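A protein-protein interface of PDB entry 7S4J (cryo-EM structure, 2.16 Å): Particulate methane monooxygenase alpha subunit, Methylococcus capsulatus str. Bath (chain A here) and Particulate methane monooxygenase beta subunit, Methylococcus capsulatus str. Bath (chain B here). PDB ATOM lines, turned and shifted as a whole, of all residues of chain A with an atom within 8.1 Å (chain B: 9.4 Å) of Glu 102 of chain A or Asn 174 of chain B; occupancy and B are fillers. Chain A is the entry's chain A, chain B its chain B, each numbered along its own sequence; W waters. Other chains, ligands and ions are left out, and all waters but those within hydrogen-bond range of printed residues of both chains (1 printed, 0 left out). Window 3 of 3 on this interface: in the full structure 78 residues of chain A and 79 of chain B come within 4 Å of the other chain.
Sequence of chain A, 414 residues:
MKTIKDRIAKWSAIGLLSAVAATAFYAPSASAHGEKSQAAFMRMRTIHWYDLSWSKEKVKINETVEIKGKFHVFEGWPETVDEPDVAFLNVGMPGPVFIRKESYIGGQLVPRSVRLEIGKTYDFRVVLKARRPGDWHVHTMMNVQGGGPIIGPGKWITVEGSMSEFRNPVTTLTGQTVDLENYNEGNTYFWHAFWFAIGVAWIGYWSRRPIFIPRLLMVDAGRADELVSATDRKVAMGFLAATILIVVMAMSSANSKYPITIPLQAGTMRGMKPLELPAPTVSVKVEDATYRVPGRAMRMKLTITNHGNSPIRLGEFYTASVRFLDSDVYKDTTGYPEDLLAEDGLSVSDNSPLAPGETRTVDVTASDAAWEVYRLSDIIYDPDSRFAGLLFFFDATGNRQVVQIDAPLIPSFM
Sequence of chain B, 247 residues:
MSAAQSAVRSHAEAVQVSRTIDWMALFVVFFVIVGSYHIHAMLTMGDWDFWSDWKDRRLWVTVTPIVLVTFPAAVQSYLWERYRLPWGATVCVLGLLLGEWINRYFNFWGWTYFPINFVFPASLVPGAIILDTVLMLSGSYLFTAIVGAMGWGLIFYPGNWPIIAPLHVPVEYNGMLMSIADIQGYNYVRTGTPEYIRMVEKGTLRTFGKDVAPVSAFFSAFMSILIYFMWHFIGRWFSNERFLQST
Among the printed residues, merely in contact across the chains: Glu 102 of chain A with Tyr 186 of chain B (3.1 Å), Ile 99 of chain A with Asn 187 of chain B (3.3 Å), Lys 101 of chain A with Tyr 186 of chain B (3.4 Å), Val 91 of chain A with Val 189 of chain B (3.4 Å), Glu 102 of chain A with Asn 174 of chain B (3.4 Å), Pro 111 of chain A with Tyr 186 of chain B (3.5 Å), Pro 111 of chain A with Met 176 of chain B (3.6 Å), Arg 100 of chain A with Val 189 of chain B (3.7 Å), Pro 111 of chain A with Met 178 of chain B (3.7 Å), Leu 109 of chain A with Tyr 173 of chain B (3.9 Å), Leu 109 of chain A with Tyr 186 of chain B (3.9 Å) and Leu 109 of chain A with Asn 174 of chain B (3.95 Å).
Printed residues of chain A that touch a printed residue of chain B: Val 91, Ile 99, Arg 100, Lys 101, Glu 102, Ser 103, Leu 109 and Pro 111.
Hydrophobic or aromatic side chains of chain A within 4 Å of the printed part of chain B: Ile 99, Leu 109 and Pro 111.
Along chain A the printed residues that touch a printed residue of chain B span positions 91 to 111.
Of the 12 printed residues of chain B, 7 touch a printed residue of chain A.
Among the printed residues, 16 pairs touch across the chains.
The backbone NH of Met 176 of chain B is in hydrogen-bond range of the side-chain carboxylate of Glu 172 of chain B, at 3.3 Å.
The backbone carbonyl oxygen of Ser 103 of chain A lies within hydrogen-bond range of the backbone NH of Val 110 of chain A (2.9 Å).
The backbone NH of Lys 101 of chain A is in hydrogen-bond range of the backbone carbonyl oxygen of Val 127 of chain A.
The side-chain carboxylate (OE1) of Glu 102 of chain A is in hydrogen-bond range of the side-chain hydroxyl (OH) of Tyr 104 of chain A (3.4 Å).
The backbone carbonyl oxygen of Glu 102 of chain A lies within hydrogen-bond range of the backbone NH of Val 127 of chain A (2.8 Å).
N of Val 171 of chain B lies within hydrogen-bond range of O of Met 178 of chain B (2.7 Å).
The backbone carbonyl oxygen of Lys 101 of chain A sits at hydrogen-bond distance from the side-chain hydroxyl of Tyr 173 of chain B (2.8 Å).
OG of Ser 103 of chain A sits at hydrogen-bond distance from OH of Tyr 186 of chain B (2.4 Å).
O of Arg 100 of chain A sits at hydrogen-bond distance from ND2 of Asn 187 of chain B (2.8 Å).
The guanidinium group (NH2) of Arg 100 of chain A is in hydrogen-bond range of the backbone carbonyl oxygen (O) of Tyr 186 of chain B (2.9 Å).
Water W1 lies within hydrogen-bond range of NZ of Lys 101 of chain A (2.4 Å), OD1 of Asn 187 of chain B (2.5 Å) and OH of Tyr 173 of chain B (3.4 Å).
Of the printed residues of chain B, Ile 99 of chain A touches Asn 187.
Of the printed residues of chain B, Arg 100 of chain A touches Tyr 186 (2.9 Å), Asn 187 (2.8 Å) and Val 189 (3.7 Å).
Of the printed residues of chain B, Glu 102 of chain A touches Asn 174 (3.4 Å) and Tyr 186 (3.1 Å).
Of the printed residues of chain B, Leu 109 of chain A touches Tyr 173, Asn 174 and Tyr 186.
No residue of chain B comes within 4 Å of Val 127 of chain A.
Asn 174 of chain B touches two residues of chain A.
Of the printed residues of chain A, Met 178 of chain B touches Pro 111.
The nearest residue of chain B that does not touch Glu 102 of chain A is Tyr 173 of chain B (5.0 Å).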
ATOM      1  N   THR A  64     -10.782   9.566  21.050  1.00  0.00           N
ATOM      2  CA  THR A  64     -11.182   8.172  20.950  1.00  0.00           C
ATOM      3  C   THR A  64     -12.659   8.016  21.286  1.00  0.00           C
ATOM      4  O   THR A  64     -13.166   8.650  22.214  1.00  0.00           O
ATOM      5  CB  THR A  64     -10.318   7.301  21.876  1.00  0.00           C
ATOM      6  OG1 THR A  64      -9.337   6.604  21.099  1.00  0.00           O
ATOM      7  CG2 THR A  64     -11.156   6.289  22.642  1.00  0.00           C
ATOM      8  N   VAL A  65     -13.350   7.194  20.502  1.00  0.00           N
ATOM      9  CA  VAL A  65     -14.710   6.764  20.797  1.00  0.00           C
ATOM     10  C   VAL A  65     -14.711   5.244  20.854  1.00  0.00           C
ATOM     11  O   VAL A  65     -14.118   4.585  19.994  1.00  0.00           O
ATOM     12  CB  VAL A  65     -15.722   7.290  19.760  1.00  0.00           C
ATOM     13  CG1 VAL A  65     -15.250   7.010  18.349  1.00  0.00           C
ATOM     14  CG2 VAL A  65     -17.093   6.683  19.993  1.00  0.00           C
ATOM     15  N   GLU A  66     -15.344   4.691  21.882  1.00  0.00           N
ATOM     16  CA  GLU A  66     -15.357   3.255  22.115  1.00  0.00           C
ATOM     17  C   GLU A  66     -16.769   2.719  21.926  1.00  0.00           C
ATOM     18  O   GLU A  66     -17.724   3.262  22.487  1.00  0.00           O
ATOM     19  CB  GLU A  66     -14.837   2.932  23.515  1.00  0.00           C
ATOM     20  CG  GLU A  66     -15.217   1.564  24.025  1.00  0.00           C
ATOM     21  CD  GLU A  66     -14.588   1.255  25.367  1.00  0.00           C
ATOM     22  OE1 GLU A  66     -13.347   1.341  25.479  1.00  0.00           O
ATOM     23  OE2 GLU A  66     -15.335   0.938  26.316  1.00  0.00           O
ATOM     24  N   ILE A  67     -16.893   1.665  21.128  1.00  0.00           N
ATOM     25  CA  ILE A  67     -18.168   1.016  20.852  1.00  0.00           C
ATOM     26  C   ILE A  67     -18.129  -0.371  21.473  1.00  0.00           C
ATOM     27  O   ILE A  67     -17.239  -1.170  21.165  1.00  0.00           O
ATOM     28  CB  ILE A  67     -18.447   0.936  19.346  1.00  0.00           C
ATOM     29  CG1 ILE A  67     -18.215   2.295  18.693  1.00  0.00           C
ATOM     30  CG2 ILE A  67     -19.859   0.445  19.092  1.00  0.00           C
ATOM     31  CD1 ILE A  67     -18.359   2.278  17.202  1.00  0.00           C
ATOM     32  N   LEU A  89     -14.340  -8.813  12.525  1.00  0.00           N
ATOM     33  CA  LEU A  89     -15.056  -7.743  13.215  1.00  0.00           C
ATOM     34  C   LEU A  89     -14.657  -6.426  12.566  1.00  0.00           C
ATOM     35  O   LEU A  89     -13.573  -5.900  12.815  1.00  0.00           O
ATOM     36  CB  LEU A  89     -14.746  -7.748  14.707  1.00  0.00           C
ATOM     37  CG  LEU A  89     -15.408  -6.636  15.523  1.00  0.00           C
ATOM     38  CD1 LEU A  89     -16.917  -6.806  15.527  1.00  0.00           C
ATOM     39  CD2 LEU A  89     -14.867  -6.598  16.940  1.00  0.00           C
ATOM     40  N   VAL A  91     -15.825  -2.358  10.900  1.00  0.00           N
ATOM     41  CA  VAL A  91     -16.560  -1.147  11.236  1.00  0.00           C
ATOM     42  C   VAL A  91     -17.136  -0.571   9.952  1.00  0.00           C
ATOM     43  O   VAL A  91     -16.426  -0.455   8.948  1.00  0.00           O
ATOM     44  CB  VAL A  91     -15.671  -0.107  11.944  1.00  0.00           C
ATOM     45  CG1 VAL A  91     -16.508   1.054  12.423  1.00  0.00           C
ATOM     46  CG2 VAL A  91     -14.932  -0.737  13.106  1.00  0.00           C
ATOM     47  N   ILE A  99      -9.927   5.805  12.450  1.00  0.00           N
ATOM     48  CA  ILE A  99      -9.031   4.664  12.346  1.00  0.00           C
ATOM     49  C   ILE A  99      -9.348   3.704  13.482  1.00  0.00           C
ATOM     50  O   ILE A  99      -9.619   4.128  14.610  1.00  0.00           O
ATOM     51  CB  ILE A  99      -7.555   5.093  12.367  1.00  0.00           C
ATOM     52  CG1 ILE A  99      -7.221   5.875  13.634  1.00  0.00           C
ATOM     53  CG2 ILE A  99      -7.216   5.890  11.121  1.00  0.00           C
ATOM     54  CD1 ILE A  99      -5.825   5.625  14.126  1.00  0.00           C
ATOM     55  N   ARG A 100      -9.353   2.412  13.176  1.00  0.00           N
ATOM     56  CA  ARG A 100      -9.583   1.383  14.183  1.00  0.00           C
ATOM     57  C   ARG A 100      -8.302   1.186  14.977  1.00  0.00           C
ATOM     58  O   ARG A 100      -7.350   0.569  14.500  1.00  0.00           O
ATOM     59  CB  ARG A 100     -10.031   0.085  13.523  1.00  0.00           C
ATOM     60  CG  ARG A 100     -10.423  -0.997  14.501  1.00  0.00           C
ATOM     61  CD  ARG A 100     -10.636  -2.327  13.807  1.00  0.00           C
ATOM     62  NE  ARG A 100     -10.003  -2.374  12.496  1.00  0.00           N
ATOM     63  CZ  ARG A 100     -10.606  -2.774  11.386  1.00  0.00           C
ATOM     64  NH1 ARG A 100     -11.870  -3.158  11.386  1.00  0.00           N
ATOM     65  NH2 ARG A 100      -9.923  -2.786  10.246  1.00  0.00           N
ATOM     66  N   LYS A 101      -8.261   1.734  16.189  1.00  0.00           N
ATOM     67  CA  LYS A 101      -7.109   1.527  17.056  1.00  0.00           C
ATOM     68  C   LYS A 101      -7.074   0.099  17.583  1.00  0.00           C
ATOM     69  O   LYS A 101      -6.041  -0.574  17.530  1.00  0.00           O
ATOM     70  CB  LYS A 101      -7.140   2.528  18.210  1.00  0.00           C
ATOM     71  CG  LYS A 101      -6.438   3.841  17.925  1.00  0.00           C
ATOM     72  CD  LYS A 101      -5.164   3.642  17.131  1.00  0.00           C
ATOM     73  CE  LYS A 101      -3.969   3.504  18.047  1.00  0.00           C
ATOM     74  NZ  LYS A 101      -2.744   3.140  17.293  1.00  0.00           N
ATOM     75  N   GLU A 102      -8.204  -0.385  18.094  1.00  0.00           N
ATOM     76  CA  GLU A 102      -8.275  -1.706  18.698  1.00  0.00           C
ATOM     77  C   GLU A 102      -9.657  -2.291  18.466  1.00  0.00           C
ATOM     78  O   GLU A 102     -10.634  -1.570  18.268  1.00  0.00           O
ATOM     79  CB  GLU A 102      -7.986  -1.662  20.201  1.00  0.00           C
ATOM     80  CG  GLU A 102      -6.549  -1.383  20.558  1.00  0.00           C
ATOM     81  CD  GLU A 102      -6.415  -0.230  21.524  1.00  0.00           C
ATOM     82  OE1 GLU A 102      -7.138  -0.219  22.540  1.00  0.00           O
ATOM     83  OE2 GLU A 102      -5.591   0.670  21.262  1.00  0.00           O
ATOM     84  N   SER A 103      -9.724  -3.617  18.502  1.00  0.00           N
ATOM     85  CA  SER A 103     -10.996  -4.321  18.436  1.00  0.00           C
ATOM     86  C   SER A 103     -10.845  -5.636  19.178  1.00  0.00           C
ATOM     87  O   SER A 103      -9.841  -6.330  19.013  1.00  0.00           O
ATOM     88  CB  SER A 103     -11.438  -4.557  16.988  1.00  0.00           C
ATOM     89  OG  SER A 103     -10.418  -5.169  16.228  1.00  0.00           O
ATOM     90  N   TYR A 104     -11.835  -5.964  20.000  1.00  0.00           N
ATOM     91  CA  TYR A 104     -11.781  -7.139  20.855  1.00  0.00           C
ATOM     92  C   TYR A 104     -13.032  -7.977  20.674  1.00  0.00           C
ATOM     93  O   TYR A 104     -14.136  -7.444  20.560  1.00  0.00           O
ATOM     94  CB  TYR A 104     -11.648  -6.755  22.329  1.00  0.00           C
ATOM     95  CG  TYR A 104     -10.465  -5.880  22.646  1.00  0.00           C
ATOM     96  CD1 TYR A 104     -10.534  -4.504  22.494  1.00  0.00           C
ATOM     97  CD2 TYR A 104      -9.278  -6.428  23.106  1.00  0.00           C
ATOM     98  CE1 TYR A 104      -9.456  -3.703  22.785  1.00  0.00           C
ATOM     99  CE2 TYR A 104      -8.194  -5.633  23.399  1.00  0.00           C
ATOM    100  CZ  TYR A 104      -8.289  -4.272  23.238  1.00  0.00           C
ATOM    101  OH  TYR A 104      -7.210  -3.474  23.530  1.00  0.00           O
ATOM    102  N   ILE A 105     -12.847  -9.291  20.640  1.00  0.00           N
ATOM    103  CA  ILE A 105     -13.932 -10.251  20.789  1.00  0.00           C
ATOM    104  C   ILE A 105     -13.663 -11.008  22.076  1.00  0.00           C
ATOM    105  O   ILE A 105     -12.619 -11.656  22.215  1.00  0.00           O
ATOM    106  CB  ILE A 105     -14.024 -11.213  19.597  1.00  0.00           C
ATOM    107  CG1 ILE A 105     -14.294 -10.451  18.301  1.00  0.00           C
ATOM    108  CG2 ILE A 105     -15.106 -12.248  19.846  1.00  0.00           C
ATOM    109  CD1 ILE A 105     -15.669  -9.891  18.211  1.00  0.00           C
ATOM    110  N   GLN A 108      -9.996 -10.098  24.025  1.00  0.00           N
ATOM    111  CA  GLN A 108      -8.708 -10.236  23.369  1.00  0.00           C
ATOM    112  C   GLN A 108      -8.717  -9.584  21.991  1.00  0.00           C
ATOM    113  O   GLN A 108      -9.715  -9.639  21.270  1.00  0.00           O
ATOM    114  CB  GLN A 108      -8.323 -11.709  23.271  1.00  0.00           C
ATOM    115  CG  GLN A 108      -9.112 -12.513  22.278  1.00  0.00           C
ATOM    116  CD  GLN A 108      -8.259 -13.561  21.610  1.00  0.00           C
ATOM    117  OE1 GLN A 108      -7.299 -13.241  20.916  1.00  0.00           O
ATOM    118  NE2 GLN A 108      -8.601 -14.827  21.823  1.00  0.00           N
ATOM    119  N   LEU A 109      -7.594  -8.961  21.643  1.00  0.00           N
ATOM    120  CA  LEU A 109      -7.496  -8.199  20.407  1.00  0.00           C
ATOM    121  C   LEU A 109      -7.625  -9.113  19.197  1.00  0.00           C
ATOM    122  O   LEU A 109      -7.054 -10.203  19.160  1.00  0.00           O
ATOM    123  CB  LEU A 109      -6.168  -7.445  20.365  1.00  0.00           C
ATOM    124  CG  LEU A 109      -6.018  -6.394  19.270  1.00  0.00           C
ATOM    125  CD1 LEU A 109      -6.357  -5.025  19.822  1.00  0.00           C
ATOM    126  CD2 LEU A 109      -4.613  -6.411  18.705  1.00  0.00           C
ATOM    127  N   VAL A 110      -8.372  -8.659  18.197  1.00  0.00           N
ATOM    128  CA  VAL A 110      -8.653  -9.492  17.031  1.00  0.00           C
ATOM    129  C   VAL A 110      -8.320  -8.738  15.748  1.00  0.00           C
ATOM    130  O   VAL A 110      -9.226  -8.377  14.986  1.00  0.00           O
ATOM    131  CB  VAL A 110     -10.114  -9.977  17.042  1.00  0.00           C
ATOM    132  CG1 VAL A 110     -10.279 -11.094  18.051  1.00  0.00           C
ATOM    133  CG2 VAL A 110     -11.062  -8.840  17.380  1.00  0.00           C
ATOM    134  N   PRO A 111      -7.039  -8.495  15.454  1.00  0.00           N
ATOM    135  CA  PRO A 111      -6.697  -7.836  14.188  1.00  0.00           C
ATOM    136  C   PRO A 111      -6.845  -8.731  12.972  1.00  0.00           C
ATOM    137  O   PRO A 111      -6.855  -8.216  11.849  1.00  0.00           O
ATOM    138  CB  PRO A 111      -5.237  -7.426  14.396  1.00  0.00           C
ATOM    139  CG  PRO A 111      -4.709  -8.449  15.318  1.00  0.00           C
ATOM    140  CD  PRO A 111      -5.839  -8.847  16.228  1.00  0.00           C
ATOM    141  N   ARG A 125     -15.668  -5.065  21.594  1.00  0.00           N
ATOM    142  CA  ARG A 125     -15.298  -3.689  21.898  1.00  0.00           C
ATOM    143  C   ARG A 125     -14.409  -3.175  20.779  1.00  0.00           C
ATOM    144  O   ARG A 125     -13.402  -3.804  20.452  1.00  0.00           O
ATOM    145  CB  ARG A 125     -14.589  -3.604  23.246  1.00  0.00           C
ATOM    146  CG  ARG A 125     -14.109  -2.223  23.617  1.00  0.00           C
ATOM    147  CD  ARG A 125     -13.835  -2.155  25.101  1.00  0.00           C
ATOM    148  NE  ARG A 125     -12.547  -2.745  25.436  1.00  0.00           N
ATOM    149  CZ  ARG A 125     -11.403  -2.080  25.476  1.00  0.00           C
ATOM    150  NH1 ARG A 125     -11.348  -0.782  25.228  1.00  0.00           N
ATOM    151  NH2 ARG A 125     -10.285  -2.732  25.778  1.00  0.00           N
ATOM    152  N   VAL A 126     -14.782  -2.043  20.192  1.00  0.00           N
ATOM    153  CA  VAL A 126     -14.013  -1.413  19.126  1.00  0.00           C
ATOM    154  C   VAL A 126     -13.622  -0.018  19.584  1.00  0.00           C
ATOM    155  O   VAL A 126     -14.475   0.748  20.043  1.00  0.00           O
ATOM    156  CB  VAL A 126     -14.804  -1.353  17.807  1.00  0.00           C
ATOM    157  CG1 VAL A 126     -13.974  -0.690  16.729  1.00  0.00           C
ATOM    158  CG2 VAL A 126     -15.221  -2.740  17.373  1.00  0.00           C
ATOM    159  N   VAL A 127     -12.341   0.308  19.462  1.00  0.00           N
ATOM    160  CA  VAL A 127     -11.827   1.627  19.807  1.00  0.00           C
ATOM    161  C   VAL A 127     -11.472   2.342  18.513  1.00  0.00           C
ATOM    162  O   VAL A 127     -10.689   1.831  17.705  1.00  0.00           O
ATOM    163  CB  VAL A 127     -10.614   1.538  20.744  1.00  0.00           C
ATOM    164  CG1 VAL A 127     -10.153   2.925  21.138  1.00  0.00           C
ATOM    165  CG2 VAL A 127     -10.961   0.720  21.974  1.00  0.00           C
ATOM    166  N   LEU A 128     -12.049   3.520  18.315  1.00  0.00           N
ATOM    167  CA  LEU A 128     -11.837   4.316  17.117  1.00  0.00           C
ATOM    168  C   LEU A 128     -11.192   5.638  17.493  1.00  0.00           C
ATOM    169  O   LEU A 128     -11.496   6.207  18.543  1.00  0.00           O
ATOM    170  CB  LEU A 128     -13.154   4.576  16.384  1.00  0.00           C
ATOM    171  CG  LEU A 128     -13.962   3.355  15.952  1.00  0.00           C
ATOM    172  CD1 LEU A 128     -15.266   3.788  15.320  1.00  0.00           C
ATOM    173  CD2 LEU A 128     -13.160   2.497  14.997  1.00  0.00           C
ATOM    174  N   LYS A 129     -10.297   6.118  16.641  1.00  0.00           N
ATOM    175  CA  LYS A 129      -9.680   7.426  16.799  1.00  0.00           C
ATOM    176  C   LYS A 129     -10.129   8.324  15.655  1.00  0.00           C
ATOM    177  O   LYS A 129      -9.997   7.953  14.485  1.00  0.00           O
ATOM    178  CB  LYS A 129      -8.157   7.313  16.833  1.00  0.00           C
ATOM    179  CG  LYS A 129      -7.457   8.612  17.146  1.00  0.00           C
ATOM    180  CD  LYS A 129      -5.983   8.525  16.832  1.00  0.00           C
ATOM    181  CE  LYS A 129      -5.144   9.038  17.977  1.00  0.00           C
ATOM    182  NZ  LYS A 129      -3.818   9.509  17.508  1.00  0.00           N
ATOM    183  N   VAL B 171       6.396  -4.664  14.774  1.00  0.00           N
ATOM    184  CA  VAL B 171       5.838  -3.787  15.796  1.00  0.00           C
ATOM    185  C   VAL B 171       5.099  -4.635  16.820  1.00  0.00           C
ATOM    186  O   VAL B 171       4.391  -5.582  16.467  1.00  0.00           O
ATOM    187  CB  VAL B 171       4.891  -2.725  15.198  1.00  0.00           C
ATOM    188  CG1 VAL B 171       4.240  -1.914  16.305  1.00  0.00           C
ATOM    189  CG2 VAL B 171       5.633  -1.810  14.247  1.00  0.00           C
ATOM    190  N   GLU B 172       5.279  -4.296  18.090  1.00  0.00           N
ATOM    191  CA  GLU B 172       4.478  -4.847  19.179  1.00  0.00           C
ATOM    192  C   GLU B 172       3.214  -4.006  19.288  1.00  0.00           C
ATOM    193  O   GLU B 172       3.244  -2.884  19.797  1.00  0.00           O
ATOM    194  CB  GLU B 172       5.275  -4.825  20.476  1.00  0.00           C
ATOM    195  CG  GLU B 172       5.107  -6.041  21.339  1.00  0.00           C
ATOM    196  CD  GLU B 172       3.672  -6.296  21.693  1.00  0.00           C
ATOM    197  OE1 GLU B 172       3.016  -5.381  22.234  1.00  0.00           O
ATOM    198  OE2 GLU B 172       3.197  -7.415  21.426  1.00  0.00           O
ATOM    199  N   TYR B 173       2.096  -4.534  18.803  1.00  0.00           N
ATOM    200  CA  TYR B 173       0.844  -3.783  18.734  1.00  0.00           C
ATOM    201  C   TYR B 173      -0.191  -4.456  19.627  1.00  0.00           C
ATOM    202  O   TYR B 173      -0.822  -5.436  19.221  1.00  0.00           O
ATOM    203  CB  TYR B 173       0.352  -3.678  17.296  1.00  0.00           C
ATOM    204  CG  TYR B 173      -0.694  -2.609  17.088  1.00  0.00           C
ATOM    205  CD1 TYR B 173      -0.331  -1.282  16.928  1.00  0.00           C
ATOM    206  CD2 TYR B 173      -2.041  -2.929  17.048  1.00  0.00           C
ATOM    207  CE1 TYR B 173      -1.277  -0.306  16.738  1.00  0.00           C
ATOM    208  CE2 TYR B 173      -2.996  -1.957  16.857  1.00  0.00           C
ATOM    209  CZ  TYR B 173      -2.608  -0.648  16.702  1.00  0.00           C
ATOM    210  OH  TYR B 173      -3.554   0.325  16.511  1.00  0.00           O
ATOM    211  N   ASN B 174      -0.363  -3.919  20.834  1.00  0.00           N
ATOM    212  CA  ASN B 174      -1.373  -4.395  21.779  1.00  0.00           C
ATOM    213  C   ASN B 174      -1.239  -5.892  22.041  1.00  0.00           C
ATOM    214  O   ASN B 174      -2.223  -6.631  22.062  1.00  0.00           O
ATOM    215  CB  ASN B 174      -2.781  -4.051  21.294  1.00  0.00           C
ATOM    216  CG  ASN B 174      -3.044  -2.565  21.286  1.00  0.00           C
ATOM    217  OD1 ASN B 174      -3.173  -1.949  20.230  1.00  0.00           O
ATOM    218  ND2 ASN B 174      -3.131  -1.976  22.469  1.00  0.00           N
ATOM    219  N   GLY B 175      -0.003  -6.345  22.231  1.00  0.00           N
ATOM    220  CA  GLY B 175       0.263  -7.721  22.580  1.00  0.00           C
ATOM    221  C   GLY B 175       0.464  -8.668  21.418  1.00  0.00           C
ATOM    222  O   GLY B 175       0.830  -9.826  21.646  1.00  0.00           O
ATOM    223  N   MET B 176       0.251  -8.223  20.186  1.00  0.00           N
ATOM    224  CA  MET B 176       0.410  -9.067  19.013  1.00  0.00           C
ATOM    225  C   MET B 176       1.522  -8.522  18.131  1.00  0.00           C
ATOM    226  O   MET B 176       1.739  -7.309  18.066  1.00  0.00           O
ATOM    227  CB  MET B 176      -0.891  -9.152  18.214  1.00  0.00           C
ATOM    228  CG  MET B 176      -1.854 -10.212  18.714  1.00  0.00           C
ATOM    229  SD  MET B 176      -2.994 -10.785  17.443  1.00  0.00           S
ATOM    230  CE  MET B 176      -2.350 -12.421  17.117  1.00  0.00           C
ATOM    231  N   LEU B 177       2.230  -9.423  17.459  1.00  0.00           N
ATOM    232  CA  LEU B 177       3.266  -9.019  16.522  1.00  0.00           C
ATOM    233  C   LEU B 177       2.620  -8.642  15.197  1.00  0.00           C
ATOM    234  O   LEU B 177       1.838  -9.416  14.639  1.00  0.00           O
ATOM    235  CB  LEU B 177       4.288 -10.132  16.320  1.00  0.00           C
ATOM    236  CG  LEU B 177       5.346  -9.783  15.273  1.00  0.00           C
ATOM    237  CD1 LEU B 177       6.273  -8.713  15.804  1.00  0.00           C
ATOM    238  CD2 LEU B 177       6.130 -10.998  14.837  1.00  0.00           C
ATOM    239  N   MET B 178       2.940  -7.453  14.700  1.00  0.00           N
ATOM    240  CA  MET B 178       2.433  -6.991  13.421  1.00  0.00           C
ATOM    241  C   MET B 178       3.533  -6.233  12.698  1.00  0.00           C
ATOM    242  O   MET B 178       4.377  -5.591  13.321  1.00  0.00           O
ATOM    243  CB  MET B 178       1.201  -6.089  13.594  1.00  0.00           C
ATOM    244  CG  MET B 178      -0.044  -6.816  14.070  1.00  0.00           C
ATOM    245  SD  MET B 178      -1.364  -5.709  14.583  1.00  0.00           S
ATOM    246  CE  MET B 178      -2.280  -5.559  13.058  1.00  0.00           C
ATOM    247  N   ILE B 183      -0.443  -3.076  10.406  1.00  0.00           N
ATOM    248  CA  ILE B 183      -1.086  -2.041  11.205  1.00  0.00           C
ATOM    249  C   ILE B 183      -1.800  -1.036  10.313  1.00  0.00           C
ATOM    250  O   ILE B 183      -2.861  -0.523  10.670  1.00  0.00           O
ATOM    251  CB  ILE B 183      -0.065  -1.358  12.128  1.00  0.00           C
ATOM    252  CG1 ILE B 183       0.543  -2.384  13.074  1.00  0.00           C
ATOM    253  CG2 ILE B 183      -0.724  -0.262  12.934  1.00  0.00           C
ATOM    254  CD1 ILE B 183       1.759  -1.887  13.754  1.00  0.00           C
ATOM    255  N   TYR B 186      -4.993  -2.662   9.461  1.00  0.00           N
ATOM    256  CA  TYR B 186      -5.865  -2.720  10.626  1.00  0.00           C
ATOM    257  C   TYR B 186      -6.484  -1.360  10.932  1.00  0.00           C
ATOM    258  O   TYR B 186      -7.685  -1.267  11.200  1.00  0.00           O
ATOM    259  CB  TYR B 186      -5.078  -3.238  11.827  1.00  0.00           C
ATOM    260  CG  TYR B 186      -5.911  -3.481  13.056  1.00  0.00           C
ATOM    261  CD1 TYR B 186      -7.052  -4.266  12.999  1.00  0.00           C
ATOM    262  CD2 TYR B 186      -5.557  -2.928  14.274  1.00  0.00           C
ATOM    263  CE1 TYR B 186      -7.813  -4.494  14.119  1.00  0.00           C
ATOM    264  CE2 TYR B 186      -6.314  -3.150  15.400  1.00  0.00           C
ATOM    265  CZ  TYR B 186      -7.439  -3.935  15.317  1.00  0.00           C
ATOM    266  OH  TYR B 186      -8.197  -4.158  16.438  1.00  0.00           O
ATOM    267  N   ASN B 187      -5.684  -0.298  10.894  1.00  0.00           N
ATOM    268  CA  ASN B 187      -6.132   1.041  11.253  1.00  0.00           C
ATOM    269  C   ASN B 187      -7.064   1.628  10.208  1.00  0.00           C
ATOM    270  O   ASN B 187      -8.190   2.015  10.526  1.00  0.00           O
ATOM    271  CB  ASN B 187      -4.938   1.977  11.442  1.00  0.00           C
ATOM    272  CG  ASN B 187      -4.182   1.712  12.719  1.00  0.00           C
ATOM    273  OD1 ASN B 187      -3.107   2.258  12.933  1.00  0.00           O
ATOM    274  ND2 ASN B 187      -4.741   0.877  13.579  1.00  0.00           N
ATOM    275  N   VAL B 189      -9.684   1.657   7.928  1.00  0.00           N
ATOM    276  CA  VAL B 189     -10.742   0.670   7.786  1.00  0.00           C
ATOM    277  C   VAL B 189     -11.219   0.612   6.344  1.00  0.00           C
ATOM    278  O   VAL B 189     -11.543   1.637   5.734  1.00  0.00           O
ATOM    279  CB  VAL B 189     -11.902   0.997   8.738  1.00  0.00           C
ATOM    280  CG1 VAL B 189     -13.072   0.066   8.491  1.00  0.00           C
ATOM    281  CG2 VAL B 189     -11.439   0.909  10.179  1.00  0.00           C
HETATM  282  O   HOH W   1      -1.899   2.886  15.011  1.00  0.00           O
